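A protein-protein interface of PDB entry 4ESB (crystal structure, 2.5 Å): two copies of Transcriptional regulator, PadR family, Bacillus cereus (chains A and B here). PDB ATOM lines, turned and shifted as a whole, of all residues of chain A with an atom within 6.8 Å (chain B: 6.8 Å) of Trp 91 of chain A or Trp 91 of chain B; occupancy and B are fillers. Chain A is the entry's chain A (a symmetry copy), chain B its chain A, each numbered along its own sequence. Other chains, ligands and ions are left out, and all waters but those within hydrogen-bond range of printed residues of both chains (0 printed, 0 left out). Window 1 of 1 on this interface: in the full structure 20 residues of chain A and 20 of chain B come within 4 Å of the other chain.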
ATOM      1  N   GLN A   4      39.306  -6.905 -28.079  1.00  0.00           N
ATOM      2  CA  GLN A   4      39.844  -8.248 -27.884  1.00  0.00           C
ATOM      3  C   GLN A   4      38.795  -9.222 -27.348  1.00  0.00           C
ATOM      4  O   GLN A   4      38.884 -10.431 -27.565  1.00  0.00           O
ATOM      5  CB  GLN A   4      41.036  -8.201 -26.922  1.00  0.00           C
ATOM      6  CG  GLN A   4      40.670  -7.844 -25.485  1.00  0.00           C
ATOM      7  CD  GLN A   4      40.026  -6.474 -25.360  1.00  0.00           C
ATOM      8  OE1 GLN A   4      39.957  -5.716 -26.329  1.00  0.00           O
ATOM      9  NE2 GLN A   4      39.551  -6.151 -24.164  1.00  0.00           N
ATOM     10  N   MET A   5      37.804  -8.686 -26.645  1.00  0.00           N
ATOM     11  CA  MET A   5      36.786  -9.502 -25.996  1.00  0.00           C
ATOM     12  C   MET A   5      35.565  -9.664 -26.895  1.00  0.00           C
ATOM     13  O   MET A   5      34.880 -10.688 -26.852  1.00  0.00           O
ATOM     14  CB  MET A   5      36.391  -8.853 -24.671  1.00  0.00           C
ATOM     15  CG  MET A   5      35.444  -9.668 -23.809  1.00  0.00           C
ATOM     16  SD  MET A   5      35.007  -8.782 -22.298  1.00  0.00           S
ATOM     17  CE  MET A   5      36.622  -8.285 -21.716  1.00  0.00           C
ATOM     18  N   VAL A   9      32.803 -13.497 -28.015  1.00  0.00           N
ATOM     19  CA  VAL A   9      31.368 -13.729 -28.123  1.00  0.00           C
ATOM     20  C   VAL A   9      30.837 -13.575 -29.548  1.00  0.00           C
ATOM     21  O   VAL A   9      29.633 -13.673 -29.779  1.00  0.00           O
ATOM     22  CB  VAL A   9      30.594 -12.738 -27.233  1.00  0.00           C
ATOM     23  CG1 VAL A   9      31.050 -12.854 -25.786  1.00  0.00           C
ATOM     24  CG2 VAL A   9      30.780 -11.315 -27.745  1.00  0.00           C
ATOM     25  N   GLU A  86      24.268 -23.666 -25.797  1.00  0.00           N
ATOM     26  CA  GLU A  86      25.371 -23.641 -24.844  1.00  0.00           C
ATOM     27  C   GLU A  86      25.853 -22.208 -24.632  1.00  0.00           C
ATOM     28  O   GLU A  86      26.098 -21.791 -23.501  1.00  0.00           O
ATOM     29  CB  GLU A  86      26.527 -24.513 -25.336  1.00  0.00           C
ATOM     30  CG  GLU A  86      26.202 -25.995 -25.407  1.00  0.00           C
ATOM     31  CD  GLU A  86      27.268 -26.788 -26.138  1.00  0.00           C
ATOM     32  OE1 GLU A  86      28.323 -26.204 -26.468  1.00  0.00           O
ATOM     33  OE2 GLU A  86      27.053 -27.994 -26.383  1.00  0.00           O
ATOM     34  N   PHE A  87      25.985 -21.455 -25.722  1.00  0.00           N
ATOM     35  CA  PHE A  87      26.443 -20.070 -25.640  1.00  0.00           C
ATOM     36  C   PHE A  87      25.464 -19.193 -24.864  1.00  0.00           C
ATOM     37  O   PHE A  87      25.873 -18.381 -24.035  1.00  0.00           O
ATOM     38  CB  PHE A  87      26.663 -19.487 -27.038  1.00  0.00           C
ATOM     39  CG  PHE A  87      26.906 -18.005 -27.039  1.00  0.00           C
ATOM     40  CD1 PHE A  87      28.128 -17.493 -26.635  1.00  0.00           C
ATOM     41  CD2 PHE A  87      25.914 -17.124 -27.437  1.00  0.00           C
ATOM     42  CE1 PHE A  87      28.357 -16.132 -26.629  1.00  0.00           C
ATOM     43  CE2 PHE A  87      26.137 -15.759 -27.434  1.00  0.00           C
ATOM     44  CZ  PHE A  87      27.361 -15.262 -27.030  1.00  0.00           C
ATOM     45  N   LYS A  88      24.173 -19.352 -25.138  1.00  0.00           N
ATOM     46  CA  LYS A  88      23.148 -18.568 -24.454  1.00  0.00           C
ATOM     47  C   LYS A  88      23.172 -18.823 -22.955  1.00  0.00           C
ATOM     48  O   LYS A  88      22.977 -17.904 -22.159  1.00  0.00           O
ATOM     49  CB  LYS A  88      21.761 -18.886 -25.014  1.00  0.00           C
ATOM     50  CG  LYS A  88      21.557 -18.384 -26.431  1.00  0.00           C
ATOM     51  CD  LYS A  88      20.170 -18.713 -26.963  1.00  0.00           C
ATOM     52  CE  LYS A  88      19.985 -18.168 -28.376  1.00  0.00           C
ATOM     53  NZ  LYS A  88      18.670 -18.525 -28.980  1.00  0.00           N
ATOM     54  N   GLN A  89      23.416 -20.072 -22.570  1.00  0.00           N
ATOM     55  CA  GLN A  89      23.449 -20.436 -21.162  1.00  0.00           C
ATOM     56  C   GLN A  89      24.689 -19.867 -20.495  1.00  0.00           C
ATOM     57  O   GLN A  89      24.598 -19.215 -19.456  1.00  0.00           O
ATOM     58  CB  GLN A  89      23.406 -21.955 -21.007  1.00  0.00           C
ATOM     59  CG  GLN A  89      22.013 -22.527 -21.175  1.00  0.00           C
ATOM     60  CD  GLN A  89      22.023 -24.009 -21.487  1.00  0.00           C
ATOM     61  OE1 GLN A  89      23.001 -24.707 -21.217  1.00  0.00           O
ATOM     62  NE2 GLN A  89      20.932 -24.497 -22.070  1.00  0.00           N
ATOM     63  N   SER A  90      25.850 -20.112 -21.095  1.00  0.00           N
ATOM     64  CA  SER A  90      27.100 -19.581 -20.571  1.00  0.00           C
ATOM     65  C   SER A  90      27.026 -18.061 -20.461  1.00  0.00           C
ATOM     66  O   SER A  90      27.411 -17.492 -19.441  1.00  0.00           O
ATOM     67  CB  SER A  90      28.278 -19.969 -21.469  1.00  0.00           C
ATOM     68  OG  SER A  90      28.278 -21.355 -21.759  1.00  0.00           O
ATOM     69  N   TRP A  91      26.524 -17.407 -21.505  1.00  0.00           N
ATOM     70  CA  TRP A  91      26.511 -15.947 -21.539  1.00  0.00           C
ATOM     71  C   TRP A  91      25.667 -15.329 -20.430  1.00  0.00           C
ATOM     72  O   TRP A  91      26.069 -14.342 -19.817  1.00  0.00           O
ATOM     73  CB  TRP A  91      26.010 -15.412 -22.877  1.00  0.00           C
ATOM     74  CG  TRP A  91      25.764 -13.950 -22.776  1.00  0.00           C
ATOM     75  CD1 TRP A  91      24.556 -13.321 -22.699  1.00  0.00           C
ATOM     76  CD2 TRP A  91      26.758 -12.926 -22.682  1.00  0.00           C
ATOM     77  NE1 TRP A  91      24.738 -11.965 -22.581  1.00  0.00           N
ATOM     78  CE2 TRP A  91      26.084 -11.696 -22.568  1.00  0.00           C
ATOM     79  CE3 TRP A  91      28.157 -12.932 -22.691  1.00  0.00           C
ATOM     80  CZ2 TRP A  91      26.756 -10.481 -22.465  1.00  0.00           C
ATOM     81  CZ3 TRP A  91      28.826 -11.725 -22.592  1.00  0.00           C
ATOM     82  CH2 TRP A  91      28.126 -10.516 -22.480  1.00  0.00           C
ATOM     83  N   GLY A  92      24.487 -15.891 -20.191  1.00  0.00           N
ATOM     84  CA  GLY A  92      23.588 -15.347 -19.191  1.00  0.00           C
ATOM     85  C   GLY A  92      24.170 -15.527 -17.803  1.00  0.00           C
ATOM     86  O   GLY A  92      23.923 -14.736 -16.895  1.00  0.00           O
ATOM     87  N   MET A  93      24.958 -16.584 -17.655  1.00  0.00           N
ATOM     88  CA  MET A  93      25.619 -16.898 -16.399  1.00  0.00           C
ATOM     89  C   MET A  93      26.709 -15.868 -16.117  1.00  0.00           C
ATOM     90  O   MET A  93      26.696 -15.197 -15.086  1.00  0.00           O
ATOM     91  CB  MET A  93      26.233 -18.295 -16.496  1.00  0.00           C
ATOM     92  CG  MET A  93      26.341 -19.042 -15.182  1.00  0.00           C
ATOM     93  SD  MET A  93      26.706 -20.793 -15.436  1.00  0.00           S
ATOM     94  CE  MET A  93      25.231 -21.330 -16.308  1.00  0.00           C
ATOM     95  N   VAL A  94      27.649 -15.750 -17.049  1.00  0.00           N
ATOM     96  CA  VAL A  94      28.762 -14.815 -16.919  1.00  0.00           C
ATOM     97  C   VAL A  94      28.283 -13.364 -16.864  1.00  0.00           C
ATOM     98  O   VAL A  94      28.793 -12.565 -16.080  1.00  0.00           O
ATOM     99  CB  VAL A  94      29.762 -14.975 -18.084  1.00  0.00           C
ATOM    100  CG1 VAL A  94      29.093 -14.660 -19.416  1.00  0.00           C
ATOM    101  CG2 VAL A  94      30.977 -14.088 -17.874  1.00  0.00           C
ATOM    102  N   SER A  95      27.308 -13.028 -17.700  1.00  0.00           N
ATOM    103  CA  SER A  95      26.752 -11.682 -17.727  1.00  0.00           C
ATOM    104  C   SER A  95      26.232 -11.305 -16.346  1.00  0.00           C
ATOM    105  O   SER A  95      26.566 -10.249 -15.809  1.00  0.00           O
ATOM    106  CB  SER A  95      25.625 -11.598 -18.758  1.00  0.00           C
ATOM    107  OG  SER A  95      24.928 -10.366 -18.668  1.00  0.00           O
ATOM    108  N   THR A  96      25.413 -12.181 -15.776  1.00  0.00           N
ATOM    109  CA  THR A  96      24.846 -11.962 -14.450  1.00  0.00           C
ATOM    110  C   THR A  96      25.943 -11.845 -13.396  1.00  0.00           C
ATOM    111  O   THR A  96      25.917 -10.949 -12.554  1.00  0.00           O
ATOM    112  CB  THR A  96      23.897 -13.113 -14.064  1.00  0.00           C
ATOM    113  OG1 THR A  96      22.682 -13.005 -14.815  1.00  0.00           O
ATOM    114  CG2 THR A  96      23.572 -13.082 -12.574  1.00  0.00           C
ATOM    115  N   THR A  97      26.907 -12.757 -13.457  1.00  0.00           N
ATOM    116  CA  THR A  97      27.992 -12.806 -12.481  1.00  0.00           C
ATOM    117  C   THR A  97      28.841 -11.534 -12.501  1.00  0.00           C
ATOM    118  O   THR A  97      29.074 -10.916 -11.462  1.00  0.00           O
ATOM    119  CB  THR A  97      28.897 -14.029 -12.731  1.00  0.00           C
ATOM    120  OG1 THR A  97      28.146 -15.232 -12.521  1.00  0.00           O
ATOM    121  CG2 THR A  97      30.098 -14.021 -11.800  1.00  0.00           C
ATOM    122  N   VAL A  98      29.304 -11.146 -13.684  1.00  0.00           N
ATOM    123  CA  VAL A  98      30.160  -9.971 -13.820  1.00  0.00           C
ATOM    124  C   VAL A  98      29.402  -8.671 -13.535  1.00  0.00           C
ATOM    125  O   VAL A  98      29.913  -7.785 -12.850  1.00  0.00           O
ATOM    126  CB  VAL A  98      30.793  -9.895 -15.227  1.00  0.00           C
ATOM    127  CG1 VAL A  98      31.485  -8.551 -15.438  1.00  0.00           C
ATOM    128  CG2 VAL A  98      31.779 -11.035 -15.429  1.00  0.00           C
ATOM    129  N   ASN A  99      28.187  -8.558 -14.060  1.00  0.00           N
ATOM    130  CA  ASN A  99      27.398  -7.341 -13.885  1.00  0.00           C
ATOM    131  C   ASN A  99      27.006  -7.084 -12.434  1.00  0.00           C
ATOM    132  O   ASN A  99      26.977  -5.937 -11.994  1.00  0.00           O
ATOM    133  CB  ASN A  99      26.146  -7.367 -14.766  1.00  0.00           C
ATOM    134  CG  ASN A  99      26.424  -6.917 -16.186  1.00  0.00           C
ATOM    135  OD1 ASN A  99      27.324  -6.112 -16.427  1.00  0.00           O
ATOM    136  ND2 ASN A  99      25.648  -7.427 -17.135  1.00  0.00           N
ATOM    137  N   LEU A 102      30.400  -5.854 -10.563  1.00  0.00           N
ATOM    138  CA  LEU A 102      30.902  -4.518 -10.875  1.00  0.00           C
ATOM    139  C   LEU A 102      30.002  -3.387 -10.375  1.00  0.00           C
ATOM    140  O   LEU A 102      30.155  -2.238 -10.794  1.00  0.00           O
ATOM    141  CB  LEU A 102      31.109  -4.376 -12.387  1.00  0.00           C
ATOM    142  CG  LEU A 102      32.180  -5.278 -13.002  1.00  0.00           C
ATOM    143  CD1 LEU A 102      32.331  -5.004 -14.492  1.00  0.00           C
ATOM    144  CD2 LEU A 102      33.510  -5.095 -12.289  1.00  0.00           C
ATOM    145  N   GLN B   4      34.207 -22.104 -19.852  1.00  0.00           N
ATOM    146  CA  GLN B   4      35.302 -21.671 -20.715  1.00  0.00           C
ATOM    147  C   GLN B   4      35.369 -20.149 -20.849  1.00  0.00           C
ATOM    148  O   GLN B   4      36.432 -19.582 -21.104  1.00  0.00           O
ATOM    149  CB  GLN B   4      35.154 -22.299 -22.104  1.00  0.00           C
ATOM    150  CG  GLN B   4      33.960 -21.787 -22.903  1.00  0.00           C
ATOM    151  CD  GLN B   4      32.631 -22.057 -22.220  1.00  0.00           C
ATOM    152  OE1 GLN B   4      32.572 -22.744 -21.199  1.00  0.00           O
ATOM    153  NE2 GLN B   4      31.557 -21.517 -22.782  1.00  0.00           N
ATOM    154  N   MET B   5      34.225 -19.496 -20.678  1.00  0.00           N
ATOM    155  CA  MET B   5      34.121 -18.055 -20.868  1.00  0.00           C
ATOM    156  C   MET B   5      34.310 -17.318 -19.546  1.00  0.00           C
ATOM    157  O   MET B   5      34.817 -16.194 -19.516  1.00  0.00           O
ATOM    158  CB  MET B   5      32.759 -17.725 -21.473  1.00  0.00           C
ATOM    159  CG  MET B   5      32.561 -16.271 -21.866  1.00  0.00           C
ATOM    160  SD  MET B   5      30.901 -15.990 -22.518  1.00  0.00           S
ATOM    161  CE  MET B   5      30.774 -17.316 -23.710  1.00  0.00           C
ATOM    162  N   VAL B   9      36.845 -13.358 -18.333  1.00  0.00           N
ATOM    163  CA  VAL B   9      36.573 -12.175 -17.526  1.00  0.00           C
ATOM    164  C   VAL B   9      37.059 -12.304 -16.082  1.00  0.00           C
ATOM    165  O   VAL B   9      36.836 -11.411 -15.267  1.00  0.00           O
ATOM    166  CB  VAL B   9      35.060 -11.892 -17.479  1.00  0.00           C
ATOM    167  CG1 VAL B   9      34.507 -11.722 -18.886  1.00  0.00           C
ATOM    168  CG2 VAL B   9      34.337 -13.016 -16.747  1.00  0.00           C
ATOM    169  N   GLU B  86      40.268  -0.341 -18.458  1.00  0.00           N
ATOM    170  CA  GLU B  86      40.111  -0.893 -19.798  1.00  0.00           C
ATOM    171  C   GLU B  86      39.083  -2.023 -19.786  1.00  0.00           C
ATOM    172  O   GLU B  86      38.229  -2.100 -20.668  1.00  0.00           O
ATOM    173  CB  GLU B  86      41.449  -1.411 -20.327  1.00  0.00           C
ATOM    174  CG  GLU B  86      42.491  -0.328 -20.550  1.00  0.00           C
ATOM    175  CD  GLU B  86      43.870  -0.898 -20.820  1.00  0.00           C
ATOM    176  OE1 GLU B  86      43.985  -2.134 -20.970  1.00  0.00           O
ATOM    177  OE2 GLU B  86      44.839  -0.112 -20.883  1.00  0.00           O
ATOM    178  N   PHE B  87      39.166  -2.895 -18.784  1.00  0.00           N
ATOM    179  CA  PHE B  87      38.238  -4.018 -18.674  1.00  0.00           C
ATOM    180  C   PHE B  87      36.801  -3.549 -18.461  1.00  0.00           C
ATOM    181  O   PHE B  87      35.874  -4.073 -19.078  1.00  0.00           O
ATOM    182  CB  PHE B  87      38.650  -4.954 -17.535  1.00  0.00           C
ATOM    183  CG  PHE B  87      37.620  -5.997 -17.212  1.00  0.00           C
ATOM    184  CD1 PHE B  87      37.442  -7.090 -18.043  1.00  0.00           C
ATOM    185  CD2 PHE B  87      36.826  -5.883 -16.082  1.00  0.00           C
ATOM    186  CE1 PHE B  87      36.493  -8.051 -17.754  1.00  0.00           C
ATOM    187  CE2 PHE B  87      35.874  -6.842 -15.787  1.00  0.00           C
ATOM    188  CZ  PHE B  87      35.708  -7.927 -16.624  1.00  0.00           C
ATOM    189  N   LYS B  88      36.617  -2.568 -17.583  1.00  0.00           N
ATOM    190  CA  LYS B  88      35.286  -2.040 -17.302  1.00  0.00           C
ATOM    191  C   LYS B  88      34.656  -1.447 -18.553  1.00  0.00           C
ATOM    192  O   LYS B  88      33.453  -1.587 -18.776  1.00  0.00           O
ATOM    193  CB  LYS B  88      35.346  -0.983 -16.198  1.00  0.00           C
ATOM    194  CG  LYS B  88      35.680  -1.557 -14.835  1.00  0.00           C
ATOM    195  CD  LYS B  88      35.734  -0.485 -13.756  1.00  0.00           C
ATOM    196  CE  LYS B  88      36.040  -1.098 -12.393  1.00  0.00           C
ATOM    197  NZ  LYS B  88      36.180  -0.086 -11.308  1.00  0.00           N
ATOM    198  N   GLN B  89      35.470  -0.788 -19.370  1.00  0.00           N
ATOM    199  CA  GLN B  89      34.976  -0.167 -20.590  1.00  0.00           C
ATOM    200  C   GLN B  89      34.615  -1.226 -21.617  1.00  0.00           C
ATOM    201  O   GLN B  89      33.515  -1.214 -22.168  1.00  0.00           O
ATOM    202  CB  GLN B  89      36.019   0.795 -21.155  1.00  0.00           C
ATOM    203  CG  GLN B  89      36.052   2.125 -20.430  1.00  0.00           C
ATOM    204  CD  GLN B  89      37.346   2.881 -20.651  1.00  0.00           C
ATOM    205  OE1 GLN B  89      38.068   2.631 -21.618  1.00  0.00           O
ATOM    206  NE2 GLN B  89      37.651   3.806 -19.747  1.00  0.00           N
ATOM    207  N   SER B  90      35.543  -2.144 -21.872  1.00  0.00           N
ATOM    208  CA  SER B  90      35.293  -3.233 -22.806  1.00  0.00           C
ATOM    209  C   SER B  90      34.060  -4.024 -22.381  1.00  0.00           C
ATOM    210  O   SER B  90      33.201  -4.330 -23.207  1.00  0.00           O
ATOM    211  CB  SER B  90      36.499  -4.172 -22.884  1.00  0.00           C
ATOM    212  OG  SER B  90      37.705  -3.458 -23.088  1.00  0.00           O
ATOM    213  N   TRP B  91      33.968  -4.348 -21.093  1.00  0.00           N
ATOM    214  CA  TRP B  91      32.882  -5.195 -20.610  1.00  0.00           C
ATOM    215  C   TRP B  91      31.503  -4.575 -20.808  1.00  0.00           C
ATOM    216  O   TRP B  91      30.561  -5.261 -21.200  1.00  0.00           O
ATOM    217  CB  TRP B  91      33.043  -5.541 -19.132  1.00  0.00           C
ATOM    218  CG  TRP B  91      31.798  -6.172 -18.623  1.00  0.00           C
ATOM    219  CD1 TRP B  91      30.855  -5.603 -17.819  1.00  0.00           C
ATOM    220  CD2 TRP B  91      31.325  -7.486 -18.930  1.00  0.00           C
ATOM    221  NE1 TRP B  91      29.831  -6.490 -17.592  1.00  0.00           N
ATOM    222  CE2 TRP B  91      30.096  -7.656 -18.265  1.00  0.00           C
ATOM    223  CE3 TRP B  91      31.828  -8.540 -19.700  1.00  0.00           C
ATOM    224  CZ2 TRP B  91      29.361  -8.836 -18.342  1.00  0.00           C
ATOM    225  CZ3 TRP B  91      31.100  -9.714 -19.775  1.00  0.00           C
ATOM    226  CH2 TRP B  91      29.879  -9.853 -19.100  1.00  0.00           C
ATOM    227  N   GLY B  92      31.378  -3.286 -20.513  1.00  0.00           N
ATOM    228  CA  GLY B  92      30.096  -2.614 -20.620  1.00  0.00           C
ATOM    229  C   GLY B  92      29.668  -2.521 -22.071  1.00  0.00           C
ATOM    230  O   GLY B  92      28.482  -2.513 -22.392  1.00  0.00           O
ATOM    231  N   MET B  93      30.661  -2.456 -22.948  1.00  0.00           N
ATOM    232  CA  MET B  93      30.436  -2.384 -24.383  1.00  0.00           C
ATOM    233  C   MET B  93      29.888  -3.716 -24.886  1.00  0.00           C
ATOM    234  O   MET B  93      28.806  -3.778 -25.469  1.00  0.00           O
ATOM    235  CB  MET B  93      31.760  -2.067 -25.079  1.00  0.00           C
ATOM    236  CG  MET B  93      31.633  -1.309 -26.385  1.00  0.00           C
ATOM    237  SD  MET B  93      33.222  -0.647 -26.931  1.00  0.00           S
ATOM    238  CE  MET B  93      33.589   0.507 -25.606  1.00  0.00           C
ATOM    239  N   VAL B  94      30.647  -4.781 -24.650  1.00  0.00           N
ATOM    240  CA  VAL B  94      30.263  -6.122 -25.079  1.00  0.00           C
ATOM    241  C   VAL B  94      28.970  -6.586 -24.409  1.00  0.00           C
ATOM    242  O   VAL B  94      28.113  -7.191 -25.050  1.00  0.00           O
ATOM    243  CB  VAL B  94      31.383  -7.143 -24.781  1.00  0.00           C
ATOM    244  CG1 VAL B  94      31.647  -7.233 -23.284  1.00  0.00           C
ATOM    245  CG2 VAL B  94      31.026  -8.508 -25.344  1.00  0.00           C
ATOM    246  N   SER B  95      28.836  -6.304 -23.118  1.00  0.00           N
ATOM    247  CA  SER B  95      27.640  -6.674 -22.373  1.00  0.00           C
ATOM    248  C   SER B  95      26.406  -6.074 -23.036  1.00  0.00           C
ATOM    249  O   SER B  95      25.431  -6.773 -23.310  1.00  0.00           O
ATOM    250  CB  SER B  95      27.749  -6.191 -20.926  1.00  0.00           C
ATOM    251  OG  SER B  95      26.525  -6.352 -20.229  1.00  0.00           O
ATOM    252  N   THR B  96      26.461  -4.773 -23.294  1.00  0.00           N
ATOM    253  CA  THR B  96      25.361  -4.063 -23.937  1.00  0.00           C
ATOM    254  C   THR B  96      25.077  -4.633 -25.323  1.00  0.00           C
ATOM    255  O   THR B  96      23.926  -4.872 -25.684  1.00  0.00           O
ATOM    256  CB  THR B  96      25.680  -2.561 -24.065  1.00  0.00           C
ATOM    257  OG1 THR B  96      25.587  -1.939 -22.778  1.00  0.00           O
ATOM    258  CG2 THR B  96      24.717  -1.874 -25.027  1.00  0.00           C
ATOM    259  N   THR B  97      26.138  -4.849 -26.092  1.00  0.00           N
ATOM    260  CA  THR B  97      26.017  -5.337 -27.463  1.00  0.00           C
ATOM    261  C   THR B  97      25.369  -6.721 -27.526  1.00  0.00           C
ATOM    262  O   THR B  97      24.411  -6.934 -28.268  1.00  0.00           O
ATOM    263  CB  THR B  97      27.398  -5.387 -28.149  1.00  0.00           C
ATOM    264  OG1 THR B  97      27.923  -4.059 -28.267  1.00  0.00           O
ATOM    265  CG2 THR B  97      27.300  -6.009 -29.531  1.00  0.00           C
ATOM    266  N   VAL B  98      25.897  -7.660 -26.747  1.00  0.00           N
ATOM    267  CA  VAL B  98      25.388  -9.029 -26.754  1.00  0.00           C
ATOM    268  C   VAL B  98      23.982  -9.124 -26.154  1.00  0.00           C
ATOM    269  O   VAL B  98      23.115  -9.811 -26.692  1.00  0.00           O
ATOM    270  CB  VAL B  98      26.334  -9.985 -25.994  1.00  0.00           C
ATOM    271  CG1 VAL B  98      25.682 -11.351 -25.799  1.00  0.00           C
ATOM    272  CG2 VAL B  98      27.654 -10.129 -26.736  1.00  0.00           C
ATOM    273  N   ASN B  99      23.759  -8.436 -25.039  1.00  0.00           N
ATOM    274  CA  ASN B  99      22.466  -8.493 -24.362  1.00  0.00           C
ATOM    275  C   ASN B  99      21.330  -7.898 -25.187  1.00  0.00           C
ATOM    276  O   ASN B  99      20.211  -8.406 -25.157  1.00  0.00           O
ATOM    277  CB  ASN B  99      22.532  -7.805 -22.995  1.00  0.00           C
ATOM    278  CG  ASN B  99      23.078  -8.715 -21.912  1.00  0.00           C
ATOM    279  OD1 ASN B  99      22.922  -9.935 -21.976  1.00  0.00           O
ATOM    280  ND2 ASN B  99      23.714  -8.126 -20.906  1.00  0.00           N
ATOM    281  N   LEU B 102      20.565 -10.592 -28.135  1.00  0.00           N
ATOM    282  CA  LEU B 102      19.908 -11.842 -27.759  1.00  0.00           C
ATOM    283  C   LEU B 102      18.460 -11.665 -27.297  1.00  0.00           C
ATOM    284  O   LEU B 102      17.880 -12.576 -26.704  1.00  0.00           O
ATOM    285  CB  LEU B 102      20.711 -12.547 -26.661  1.00  0.00           C
ATOM    286  CG  LEU B 102      22.111 -13.022 -27.057  1.00  0.00           C
ATOM    287  CD1 LEU B 102      22.783 -13.754 -25.905  1.00  0.00           C
ATOM    288  CD2 LEU B 102      22.047 -13.910 -28.289  1.00  0.00           C
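The backbone carbonyl oxygen (O) of Ser 95 of chain B lies close to the side-chain amide nitrogen (ND2) of Asn 99 of chain B, 3.2 Å away. OG of Ser 90 of chain B is in hydrogen-bond range of O of Glu 86 of chain B (2.8 Å). The side-chain hydroxyl (OG) of Ser 90 of chain A sits at hydrogen-bond distance from the backbone carbonyl oxygen (O) of Glu 86 of chain A (2.8 Å). The backbone carbonyl oxygen (O) of Ser 95 of chain A sits close to the side-chain amide nitrogen (ND2) of Asn 99 of chain A, 3.3 Å away.
Gln 4 of chain A touches Ser 90 of chain B, and with the chains exchanged Ser 90 of chain A touches Gln 4 of chain B. Met 5 of chain A touches Phe 87 of chain B, and with the chains exchanged Phe 87 of chain A touches Met 5 of chain B. Trp 91 of chain A touches its own counterpart, Trp 91 of chain B. Ser 95 of chain A touches Asn 99 of chain B, and with the chains exchanged Asn 99 of chain A touches Ser 95 of chain B. Positions printed for both chains: 4, 5, 9, 86, 87, 88, 89, 90, 91, 92, 93, 94, 95, 96, 97, 98, 99 and 102. Of the 21 pairs that touch across the chains among the printed residues, 21 have their exchanged pair printed and touching as well.
The side-chain hydroxyl (OG) of Ser 90 of chain A lies within hydrogen-bond range of the side-chain amide nitrogen (NE2) of Gln 4 of chain B (3.4 Å). The side-chain amide oxygen of Asn 99 of chain A sits at hydrogen-bond distance from the indole nitrogen of Trp 91 of chain B (2.8 Å). OG of Ser 90 of chain B sits at hydrogen-bond distance from NE2 of Gln 4 of chain A (3.4 Å). The side-chain hydroxyl (OG) of Ser 95 of chain A sits at hydrogen-bond distance from the side-chain amide nitrogen (ND2) of Asn 99 of chain B, at 3.4 Å. OD1 of Asn 99 of chain B sits at hydrogen-bond distance from NE1 of Trp 91 of chain A. ND2 of Asn 99 of chain A sits at hydrogen-bond distance from OG of Ser 95 of chain B (3.4 Å).
Val 94 of chain B touches Val 9 of chain A (CG2 to CG2, 3.7 Å). Val 9 of chain A touches Val 98 of chain B. Met 5 of chain B touches Phe 87 of chain A (CE to CD1, 3.9 Å). Trp 91 of chain A touches Ser 95 of chain B. Trp 91 of chain A touches Leu 102 of chain B. Val 94 of chain A touches Met 5 of chain B. Trp 91 of chain B touches Ser 95 of chain A. CG2 of Val 9 of chain B touches CG2 of Val 98 of chain A (3.5 Å). Val 98 of chain A touches Trp 91 of chain B (CG1 to CE2, 3.3 Å). CD1 of Trp 91 of chain B touches CD1 of Leu 102 of chain A (3.7 Å).
Hydrophobic or aromatic side chains of chain B within 4 Å of the printed part of chain A: Met 5, Val 9, Phe 87, Trp 91, Val 94, Val 98 and Leu 102. Hydrophobic or aromatic side chains of chain A within 4 Å of the printed part of chain B: Met 5, Val 9, Phe 87, Trp 91, Val 94, Val 98 and Leu 102. Along chain A the printed residues that touch a printed residue of chain B span positions 4 to 102. Among the printed residues, 21 pairs touch across the chains. Among the printed residues, no Asp or Glu carboxylate lies within 4 Å of a Lys or Arg side-chain nitrogen of the other chain.
Of chain B, only Trp 91 (3.9 Å), Ser 95 (3.9 Å), Val 98 (3.3 Å), Asn 99 (2.8 Å) and Leu 102 (3.7 Å) come within 4 Å of Trp 91 of chain A. Of the printed residues of chain A, Trp 91 of chain B touches Trp 91, Ser 95, Val 98, Asn 99 and Leu 102. Printed residues of chain A within 4 Å of Phe 87 of chain B: Met 5. Of the printed residues of chain A, Ser 95 of chain B touches Trp 91 and Asn 99. Of the printed residues of chain B, Met 5 of chain A touches Phe 87 and Val 94. Of the printed residues of chain A, Val 98 of chain B touches Val 9 (3.5 Å) and Trp 91 (3.3 Å). Printed residues of chain B within 4 Å of Val 98 of chain A: Val 9 (3.5 Å) and Trp 91 (3.3 Å). Gly 92 of chain A touches none of the printed residues of chain B. Glu 86 of chain B touches none of the printed residues of chain A. The nearest residue of chain A that does not touch Trp 91 of chain B is Met 5 of chain A (4.1 Å).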
